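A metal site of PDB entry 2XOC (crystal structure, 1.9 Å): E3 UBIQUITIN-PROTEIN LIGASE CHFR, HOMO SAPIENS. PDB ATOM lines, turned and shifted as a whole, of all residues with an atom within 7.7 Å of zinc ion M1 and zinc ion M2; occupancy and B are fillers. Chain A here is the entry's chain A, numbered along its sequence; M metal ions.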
ATOM      1  N   ARG A  26       7.058  -0.353  -4.167  1.00  0.00           N
ATOM      2  CA  ARG A  26       5.706  -0.727  -4.581  1.00  0.00           C
ATOM      3  C   ARG A  26       5.438  -0.456  -6.060  1.00  0.00           C
ATOM      4  O   ARG A  26       4.732  -1.215  -6.714  1.00  0.00           O
ATOM      5  CB  ARG A  26       4.663   0.027  -3.743  1.00  0.00           C
ATOM      6  CG  ARG A  26       4.283  -0.649  -2.440  1.00  0.00           C
ATOM      7  CD  ARG A  26       3.126   0.101  -1.780  1.00  0.00           C
ATOM      8  NE  ARG A  26       3.419   0.414  -0.381  1.00  0.00           N
ATOM      9  CZ  ARG A  26       2.626   1.145   0.409  1.00  0.00           C
ATOM     10  NH1 ARG A  26       1.488   1.624  -0.066  1.00  0.00           N
ATOM     11  NH2 ARG A  26       2.974   1.386   1.665  1.00  0.00           N
ATOM     12  N   LEU A  81      13.256   7.168   1.295  1.00  0.00           N
ATOM     13  CA  LEU A  81      12.745   6.291   2.345  1.00  0.00           C
ATOM     14  C   LEU A  81      11.784   7.041   3.245  1.00  0.00           C
ATOM     15  O   LEU A  81      12.098   8.125   3.742  1.00  0.00           O
ATOM     16  CB  LEU A  81      13.885   5.713   3.171  1.00  0.00           C
ATOM     17  CG  LEU A  81      14.898   4.815   2.459  1.00  0.00           C
ATOM     18  CD1 LEU A  81      15.823   4.152   3.476  1.00  0.00           C
ATOM     19  CD2 LEU A  81      14.187   3.771   1.621  1.00  0.00           C
ATOM     20  N   CYS A  82      10.605   6.475   3.476  1.00  0.00           N
ATOM     21  CA  CYS A  82       9.665   7.060   4.415  1.00  0.00           C
ATOM     22  C   CYS A  82      10.302   7.118   5.797  1.00  0.00           C
ATOM     23  O   CYS A  82      10.864   6.131   6.263  1.00  0.00           O
ATOM     24  CB  CYS A  82       8.367   6.258   4.468  1.00  0.00           C
ATOM     25  SG  CYS A  82       7.189   6.879   5.695  1.00  0.00           S
ATOM     26  N   THR A  83      10.210   8.283   6.434  1.00  0.00           N
ATOM     27  CA  THR A  83      10.829   8.478   7.731  1.00  0.00           C
ATOM     28  C   THR A  83      10.157   7.619   8.800  1.00  0.00           C
ATOM     29  O   THR A  83      10.765   7.278   9.814  1.00  0.00           O
ATOM     30  CB  THR A  83      10.797   9.962   8.124  1.00  0.00           C
ATOM     31  OG1 THR A  83      11.484  10.735   7.134  1.00  0.00           O
ATOM     32  CG2 THR A  83      11.458  10.184   9.482  1.00  0.00           C
ATOM     33  N   CYS A  84       8.904   7.260   8.552  1.00  0.00           N
ATOM     34  CA  CYS A  84       8.135   6.470   9.506  1.00  0.00           C
ATOM     35  C   CYS A  84       8.358   4.964   9.354  1.00  0.00           C
ATOM     36  O   CYS A  84       8.789   4.289  10.292  1.00  0.00           O
ATOM     37  CB  CYS A  84       6.642   6.799   9.393  1.00  0.00           C
ATOM     38  SG  CYS A  84       5.552   5.676  10.284  1.00  0.00           S
ATOM     39  N   CYS A  85       8.068   4.432   8.170  1.00  0.00           N
ATOM     40  CA  CYS A  85       8.107   2.987   7.960  1.00  0.00           C
ATOM     41  C   CYS A  85       9.399   2.498   7.313  1.00  0.00           C
ATOM     42  O   CYS A  85       9.633   1.297   7.205  1.00  0.00           O
ATOM     43  CB  CYS A  85       6.905   2.544   7.115  1.00  0.00           C
ATOM     44  SG  CYS A  85       7.013   3.040   5.384  1.00  0.00           S
ATOM     45  N   PHE A  86      10.235   3.435   6.870  1.00  0.00           N
ATOM     46  CA  PHE A  86      11.541   3.116   6.282  1.00  0.00           C
ATOM     47  C   PHE A  86      11.473   2.444   4.904  1.00  0.00           C
ATOM     48  O   PHE A  86      12.495   2.018   4.375  1.00  0.00           O
ATOM     49  CB  PHE A  86      12.376   2.243   7.224  1.00  0.00           C
ATOM     50  CG  PHE A  86      12.341   2.682   8.655  1.00  0.00           C
ATOM     51  CD1 PHE A  86      12.892   3.887   9.048  1.00  0.00           C
ATOM     52  CD2 PHE A  86      11.762   1.869   9.623  1.00  0.00           C
ATOM     53  CE1 PHE A  86      12.865   4.287  10.365  1.00  0.00           C
ATOM     54  CE2 PHE A  86      11.722   2.262  10.941  1.00  0.00           C
ATOM     55  CZ  PHE A  86      12.279   3.471  11.322  1.00  0.00           C
ATOM     56  N   GLN A  87      10.282   2.354   4.332  1.00  0.00           N
ATOM     57  CA  GLN A  87      10.123   1.745   3.018  1.00  0.00           C
ATOM     58  C   GLN A  87      10.329   2.775   1.907  1.00  0.00           C
ATOM     59  O   GLN A  87       9.980   3.946   2.072  1.00  0.00           O
ATOM     60  CB  GLN A  87       8.758   1.075   2.880  1.00  0.00           C
ATOM     61  CG  GLN A  87       8.473   0.036   3.958  1.00  0.00           C
ATOM     62  CD  GLN A  87       9.610  -0.959   4.119  1.00  0.00           C
ATOM     63  OE1 GLN A  87       9.844  -1.802   3.255  1.00  0.00           O
ATOM     64  NE2 GLN A  87      10.337  -0.854   5.228  1.00  0.00           N
ATOM     65  N   PRO A  88      10.899   2.346   0.773  1.00  0.00           N
ATOM     66  CA  PRO A  88      11.201   3.276  -0.315  1.00  0.00           C
ATOM     67  C   PRO A  88       9.947   3.648  -1.117  1.00  0.00           C
ATOM     68  O   PRO A  88       9.042   2.832  -1.295  1.00  0.00           O
ATOM     69  CB  PRO A  88      12.164   2.480  -1.194  1.00  0.00           C
ATOM     70  CG  PRO A  88      11.740   1.067  -0.995  1.00  0.00           C
ATOM     71  CD  PRO A  88      11.315   0.972   0.456  1.00  0.00           C
ATOM     72  N   MET A  89       9.918   4.892  -1.571  1.00  0.00           N
ATOM     73  CA  MET A  89       8.881   5.363  -2.482  1.00  0.00           C
ATOM     74  C   MET A  89       9.581   6.184  -3.548  1.00  0.00           C
ATOM     75  O   MET A  89      10.689   6.676  -3.319  1.00  0.00           O
ATOM     76  CB  MET A  89       7.863   6.218  -1.744  1.00  0.00           C
ATOM     77  CG  MET A  89       8.465   7.444  -1.085  1.00  0.00           C
ATOM     78  SD  MET A  89       7.273   8.411  -0.140  1.00  0.00           S
ATOM     79  CE  MET A  89       8.335   9.672   0.552  1.00  0.00           C
ATOM     80  N   PRO A 113      10.773  13.144   4.537  1.00  0.00           N
ATOM     81  CA  PRO A 113       9.825  12.431   3.668  1.00  0.00           C
ATOM     82  C   PRO A 113       8.942  11.435   4.420  1.00  0.00           C
ATOM     83  O   PRO A 113       9.443  10.739   5.302  1.00  0.00           O
ATOM     84  CB  PRO A 113      10.750  11.689   2.701  1.00  0.00           C
ATOM     85  CG  PRO A 113      12.003  11.461   3.466  1.00  0.00           C
ATOM     86  CD  PRO A 113      12.141  12.624   4.425  1.00  0.00           C
ATOM     87  N   PHE A 114       7.661  11.391   4.064  1.00  0.00           N
ATOM     88  CA  PHE A 114       6.715  10.412   4.616  1.00  0.00           C
ATOM     89  C   PHE A 114       5.825   9.913   3.477  1.00  0.00           C
ATOM     90  O   PHE A 114       5.502  10.678   2.571  1.00  0.00           O
ATOM     91  CB  PHE A 114       5.862  11.032   5.715  1.00  0.00           C
ATOM     92  CG  PHE A 114       6.634  11.427   6.955  1.00  0.00           C
ATOM     93  CD1 PHE A 114       6.778  10.544   8.004  1.00  0.00           C
ATOM     94  CD2 PHE A 114       7.216  12.676   7.037  1.00  0.00           C
ATOM     95  CE1 PHE A 114       7.492  10.904   9.136  1.00  0.00           C
ATOM     96  CE2 PHE A 114       7.943  13.042   8.167  1.00  0.00           C
ATOM     97  CZ  PHE A 114       8.075  12.153   9.217  1.00  0.00           C
ATOM     98  N   CYS A 115       5.429   8.642   3.525  1.00  0.00           N
ATOM     99  CA  CYS A 115       4.747   8.038   2.381  1.00  0.00           C
ATOM    100  C   CYS A 115       3.225   7.981   2.470  1.00  0.00           C
ATOM    101  O   CYS A 115       2.562   7.552   1.537  1.00  0.00           O
ATOM    102  CB  CYS A 115       5.284   6.617   2.131  1.00  0.00           C
ATOM    103  SG  CYS A 115       4.541   5.348   3.193  1.00  0.00           S
ATOM    104  N   HIS A 116       2.667   8.417   3.603  1.00  0.00           N
ATOM    105  CA  HIS A 116       1.250   8.168   3.869  1.00  0.00           C
ATOM    106  C   HIS A 116       0.284   8.757   2.849  1.00  0.00           C
ATOM    107  O   HIS A 116      -0.579   8.063   2.328  1.00  0.00           O
ATOM    108  CB  HIS A 116       0.844   8.587   5.274  1.00  0.00           C
ATOM    109  CG  HIS A 116      -0.517   8.111   5.664  1.00  0.00           C
ATOM    110  ND1 HIS A 116      -0.848   6.777   5.708  1.00  0.00           N
ATOM    111  CD2 HIS A 116      -1.644   8.786   6.016  1.00  0.00           C
ATOM    112  CE1 HIS A 116      -2.111   6.640   6.075  1.00  0.00           C
ATOM    113  NE2 HIS A 116      -2.613   7.847   6.266  1.00  0.00           N
ATOM    114  N   TRP A 119       0.774   6.985  -0.902  1.00  0.00           N
ATOM    115  CA  TRP A 119       0.193   5.676  -1.183  1.00  0.00           C
ATOM    116  C   TRP A 119      -0.244   4.880   0.046  1.00  0.00           C
ATOM    117  O   TRP A 119      -0.547   3.689  -0.060  1.00  0.00           O
ATOM    118  CB  TRP A 119       1.120   4.829  -2.065  1.00  0.00           C
ATOM    119  CG  TRP A 119       2.449   4.487  -1.452  1.00  0.00           C
ATOM    120  CD1 TRP A 119       2.784   4.524  -0.140  1.00  0.00           C
ATOM    121  CD2 TRP A 119       3.610   4.021  -2.154  1.00  0.00           C
ATOM    122  NE1 TRP A 119       4.092   4.129   0.025  1.00  0.00           N
ATOM    123  CE2 TRP A 119       4.616   3.814  -1.194  1.00  0.00           C
ATOM    124  CE3 TRP A 119       3.903   3.783  -3.500  1.00  0.00           C
ATOM    125  CZ2 TRP A 119       5.895   3.370  -1.533  1.00  0.00           C
ATOM    126  CZ3 TRP A 119       5.169   3.331  -3.838  1.00  0.00           C
ATOM    127  CH2 TRP A 119       6.149   3.130  -2.864  1.00  0.00           C
ATOM    128  N   GLY A 120      -0.287   5.530   1.197  1.00  0.00           N
ATOM    129  CA  GLY A 120      -0.731   4.881   2.419  1.00  0.00           C
ATOM    130  C   GLY A 120       0.371   4.123   3.126  1.00  0.00           C
ATOM    131  O   GLY A 120       0.902   3.141   2.610  1.00  0.00           O
ATOM    132  N   CYS A 121       0.704   4.579   4.333  1.00  0.00           N
ATOM    133  CA  CYS A 121       1.766   3.974   5.114  1.00  0.00           C
ATOM    134  C   CYS A 121       1.178   2.934   6.073  1.00  0.00           C
ATOM    135  O   CYS A 121       0.052   3.090   6.546  1.00  0.00           O
ATOM    136  CB  CYS A 121       2.505   5.061   5.903  1.00  0.00           C
ATOM    137  SG  CYS A 121       3.900   4.478   6.889  1.00  0.00           S
ATOM    138  N   THR A 122       1.946   1.884   6.349  1.00  0.00           N
ATOM    139  CA  THR A 122       1.508   0.864   7.293  1.00  0.00           C
ATOM    140  C   THR A 122       2.641   0.458   8.226  1.00  0.00           C
ATOM    141  O   THR A 122       3.689   0.004   7.793  1.00  0.00           O
ATOM    142  CB  THR A 122       0.979  -0.393   6.570  1.00  0.00           C
ATOM    143  OG1 THR A 122      -0.150  -0.046   5.750  1.00  0.00           O
ATOM    144  CG2 THR A 122       0.548  -1.443   7.581  1.00  0.00           C
ATOM    145  N   ARG A 123       2.405   0.656   9.523  1.00  0.00           N
ATOM    146  CA  ARG A 123       3.352   0.239  10.543  1.00  0.00           C
ATOM    147  C   ARG A 123       2.677   0.275  11.895  1.00  0.00           C
ATOM    148  O   ARG A 123       1.849   1.157  12.155  1.00  0.00           O
ATOM    149  CB  ARG A 123       4.593   1.160  10.551  1.00  0.00           C
ATOM    150  CG  ARG A 123       5.614   0.781  11.625  1.00  0.00           C
ATOM    151  CD  ARG A 123       6.805   1.740  11.652  1.00  0.00           C
ATOM    152  NE  ARG A 123       6.424   3.077  12.107  1.00  0.00           N
ATOM    153  CZ  ARG A 123       6.342   3.435  13.385  1.00  0.00           C
ATOM    154  NH1 ARG A 123       6.602   2.558  14.348  1.00  0.00           N
ATOM    155  NH2 ARG A 123       6.003   4.680  13.702  1.00  0.00           N
ATOM    156  N   GLY A 125       2.252   1.469  15.267  1.00  0.00           N
ATOM    157  CA  GLY A 125       2.709   2.725  15.844  1.00  0.00           C
ATOM    158  C   GLY A 125       2.431   3.881  14.907  1.00  0.00           C
ATOM    159  O   GLY A 125       2.383   5.042  15.335  1.00  0.00           O
ATOM    160  N   CYS A 126       2.265   3.580  13.623  1.00  0.00           N
ATOM    161  CA  CYS A 126       1.870   4.602  12.656  1.00  0.00           C
ATOM    162  C   CYS A 126       0.353   4.771  12.644  1.00  0.00           C
ATOM    163  O   CYS A 126      -0.382   3.810  12.430  1.00  0.00           O
ATOM    164  CB  CYS A 126       2.375   4.268  11.246  1.00  0.00           C
ATOM    165  SG  CYS A 126       1.782   5.421   9.983  1.00  0.00           S
ATOM    166  N   TYR A 127      -0.098   5.997  12.875  1.00  0.00           N
ATOM    167  CA  TYR A 127      -1.522   6.300  12.892  1.00  0.00           C
ATOM    168  C   TYR A 127      -1.955   6.944  11.574  1.00  0.00           C
ATOM    169  O   TYR A 127      -3.127   7.280  11.402  1.00  0.00           O
ATOM    170  CB  TYR A 127      -1.852   7.289  14.024  1.00  0.00           C
ATOM    171  CG  TYR A 127      -1.331   6.913  15.392  1.00  0.00           C
ATOM    172  CD1 TYR A 127      -1.584   5.661  15.952  1.00  0.00           C
ATOM    173  CD2 TYR A 127      -0.599   7.827  16.154  1.00  0.00           C
ATOM    174  CE1 TYR A 127      -1.107   5.330  17.204  1.00  0.00           C
ATOM    175  CE2 TYR A 127      -0.122   7.495  17.406  1.00  0.00           C
ATOM    176  CZ  TYR A 127      -0.381   6.248  17.933  1.00  0.00           C
ATOM    177  OH  TYR A 127       0.083   5.923  19.182  1.00  0.00           O
ATOM    178  N   GLY A 128      -1.016   7.091  10.655  1.00  0.00           N
ATOM    179  CA  GLY A 128      -1.200   7.916   9.476  1.00  0.00           C
ATOM    180  C   GLY A 128      -0.269   9.113   9.612  1.00  0.00           C
ATOM    181  O   GLY A 128      -0.676  10.161  10.114  1.00  0.00           O
ATOM    182  N   CYS A 129       0.965   8.942   9.171  1.00  0.00           N
ATOM    183  CA  CYS A 129       2.082   9.787   9.586  1.00  0.00           C
ATOM    184  C   CYS A 129       2.199  11.127   8.877  1.00  0.00           C
ATOM    185  O   CYS A 129       3.050  11.943   9.228  1.00  0.00           O
ATOM    186  CB  CYS A 129       3.397   9.003   9.462  1.00  0.00           C
ATOM    187  SG  CYS A 129       3.620   8.231   7.833  1.00  0.00           S
ATOM    188  N   LEU A 130       1.347  11.371   7.885  1.00  0.00           N
ATOM    189  CA  LEU A 130       1.347  12.661   7.197  1.00  0.00           C
ATOM    190  C   LEU A 130      -0.074  13.098   6.857  1.00  0.00           C
ATOM    191  O   LEU A 130      -0.830  12.338   6.261  1.00  0.00           O
ATOM    192  CB  LEU A 130       2.180  12.571   5.917  1.00  0.00           C
ATOM    193  CG  LEU A 130       2.451  13.869   5.166  1.00  0.00           C
ATOM    194  CD1 LEU A 130       3.305  14.813   6.006  1.00  0.00           C
ATOM    195  CD2 LEU A 130       3.111  13.577   3.827  1.00  0.00           C
ATOM    196  N   TYR A 199       3.426  13.217  12.000  1.00  0.00           N
ATOM    197  CA  TYR A 199       2.983  12.892  13.344  1.00  0.00           C
ATOM    198  C   TYR A 199       3.748  13.646  14.431  1.00  0.00           C
ATOM    199  O   TYR A 199       3.137  14.276  15.292  1.00  0.00           O
ATOM    200  CB  TYR A 199       3.083  11.383  13.594  1.00  0.00           C
ATOM    201  CG  TYR A 199       3.004  11.020  15.056  1.00  0.00           C
ATOM    202  CD1 TYR A 199       1.785  11.012  15.718  1.00  0.00           C
ATOM    203  CD2 TYR A 199       4.146  10.701  15.763  1.00  0.00           C
ATOM    204  CE1 TYR A 199       1.718  10.691  17.063  1.00  0.00           C
ATOM    205  CE2 TYR A 199       4.079  10.380  17.108  1.00  0.00           C
ATOM    206  CZ  TYR A 199       2.871  10.378  17.745  1.00  0.00           C
ATOM    207  OH  TYR A 199       2.809  10.046  19.081  1.00  0.00           O
HETATM  208 ZN    ZN M   1       3.768   5.974   8.768  1.00  0.00          ZN
HETATM  209 ZN    ZN M   2       5.672   5.083   5.300  1.00  0.00          ZN
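SG of Cys 126 sits close to N of Gly 128, at 3.3 Å. The side-chain sulfur (SG) of Cys 82 lies close to the backbone NH (N) of Cys 84 (3.4 Å). N of Cys 121 lies within hydrogen-bond range of ND1 of His 116. The side-chain amide nitrogen of Gln 87 lies within hydrogen-bond range of the backbone carbonyl oxygen of Cys 85, 3.0 Å away. NE1 of Trp 119 sits close to SG of Cys 115. N of Tyr 199 sits at hydrogen-bond distance from O of Cys 129, 3.1 Å away. N of Cys 82 is in hydrogen-bond range of O of Gln 87 (3.0 Å). The backbone carbonyl oxygen (O) of Cys 84 is in hydrogen-bond range of the guanidinium group (NE) of Arg 123, 3.2 Å away.
Within 4 Å of zinc ion M1: Cys 84, Cys 121, Cys 126 and Cys 129. Along chain A the residues within 4 Å of zinc ion M1 span positions 84 to 129. The nearest printed residue that does not touch zinc ion M1 is Cys 85 (4.6 Å).
Of the 26 residues printed, 4 come within 4 Å of zinc ion M2. The nearest printed residue that does not touch zinc ion M2 is Cys 129 (4.5 Å).
Zinc ion M1 is bound by the side-chain sulfur of Cys 84 (2.4 Å), the side-chain sulfur of Cys 126 (2.4 Å), the side-chain sulfur of Cys 121 (2.4 Å) and the side-chain sulfur of Cys 129 (2.4 Å). Zinc ion M1 has four donor atoms within binding distance.
Zinc ion M2 is bound by SG of Cys 82, SG of Cys 115, SG of Cys 85 and SG of Cys 121. Zinc ion M2 has four donor atoms within binding distance.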
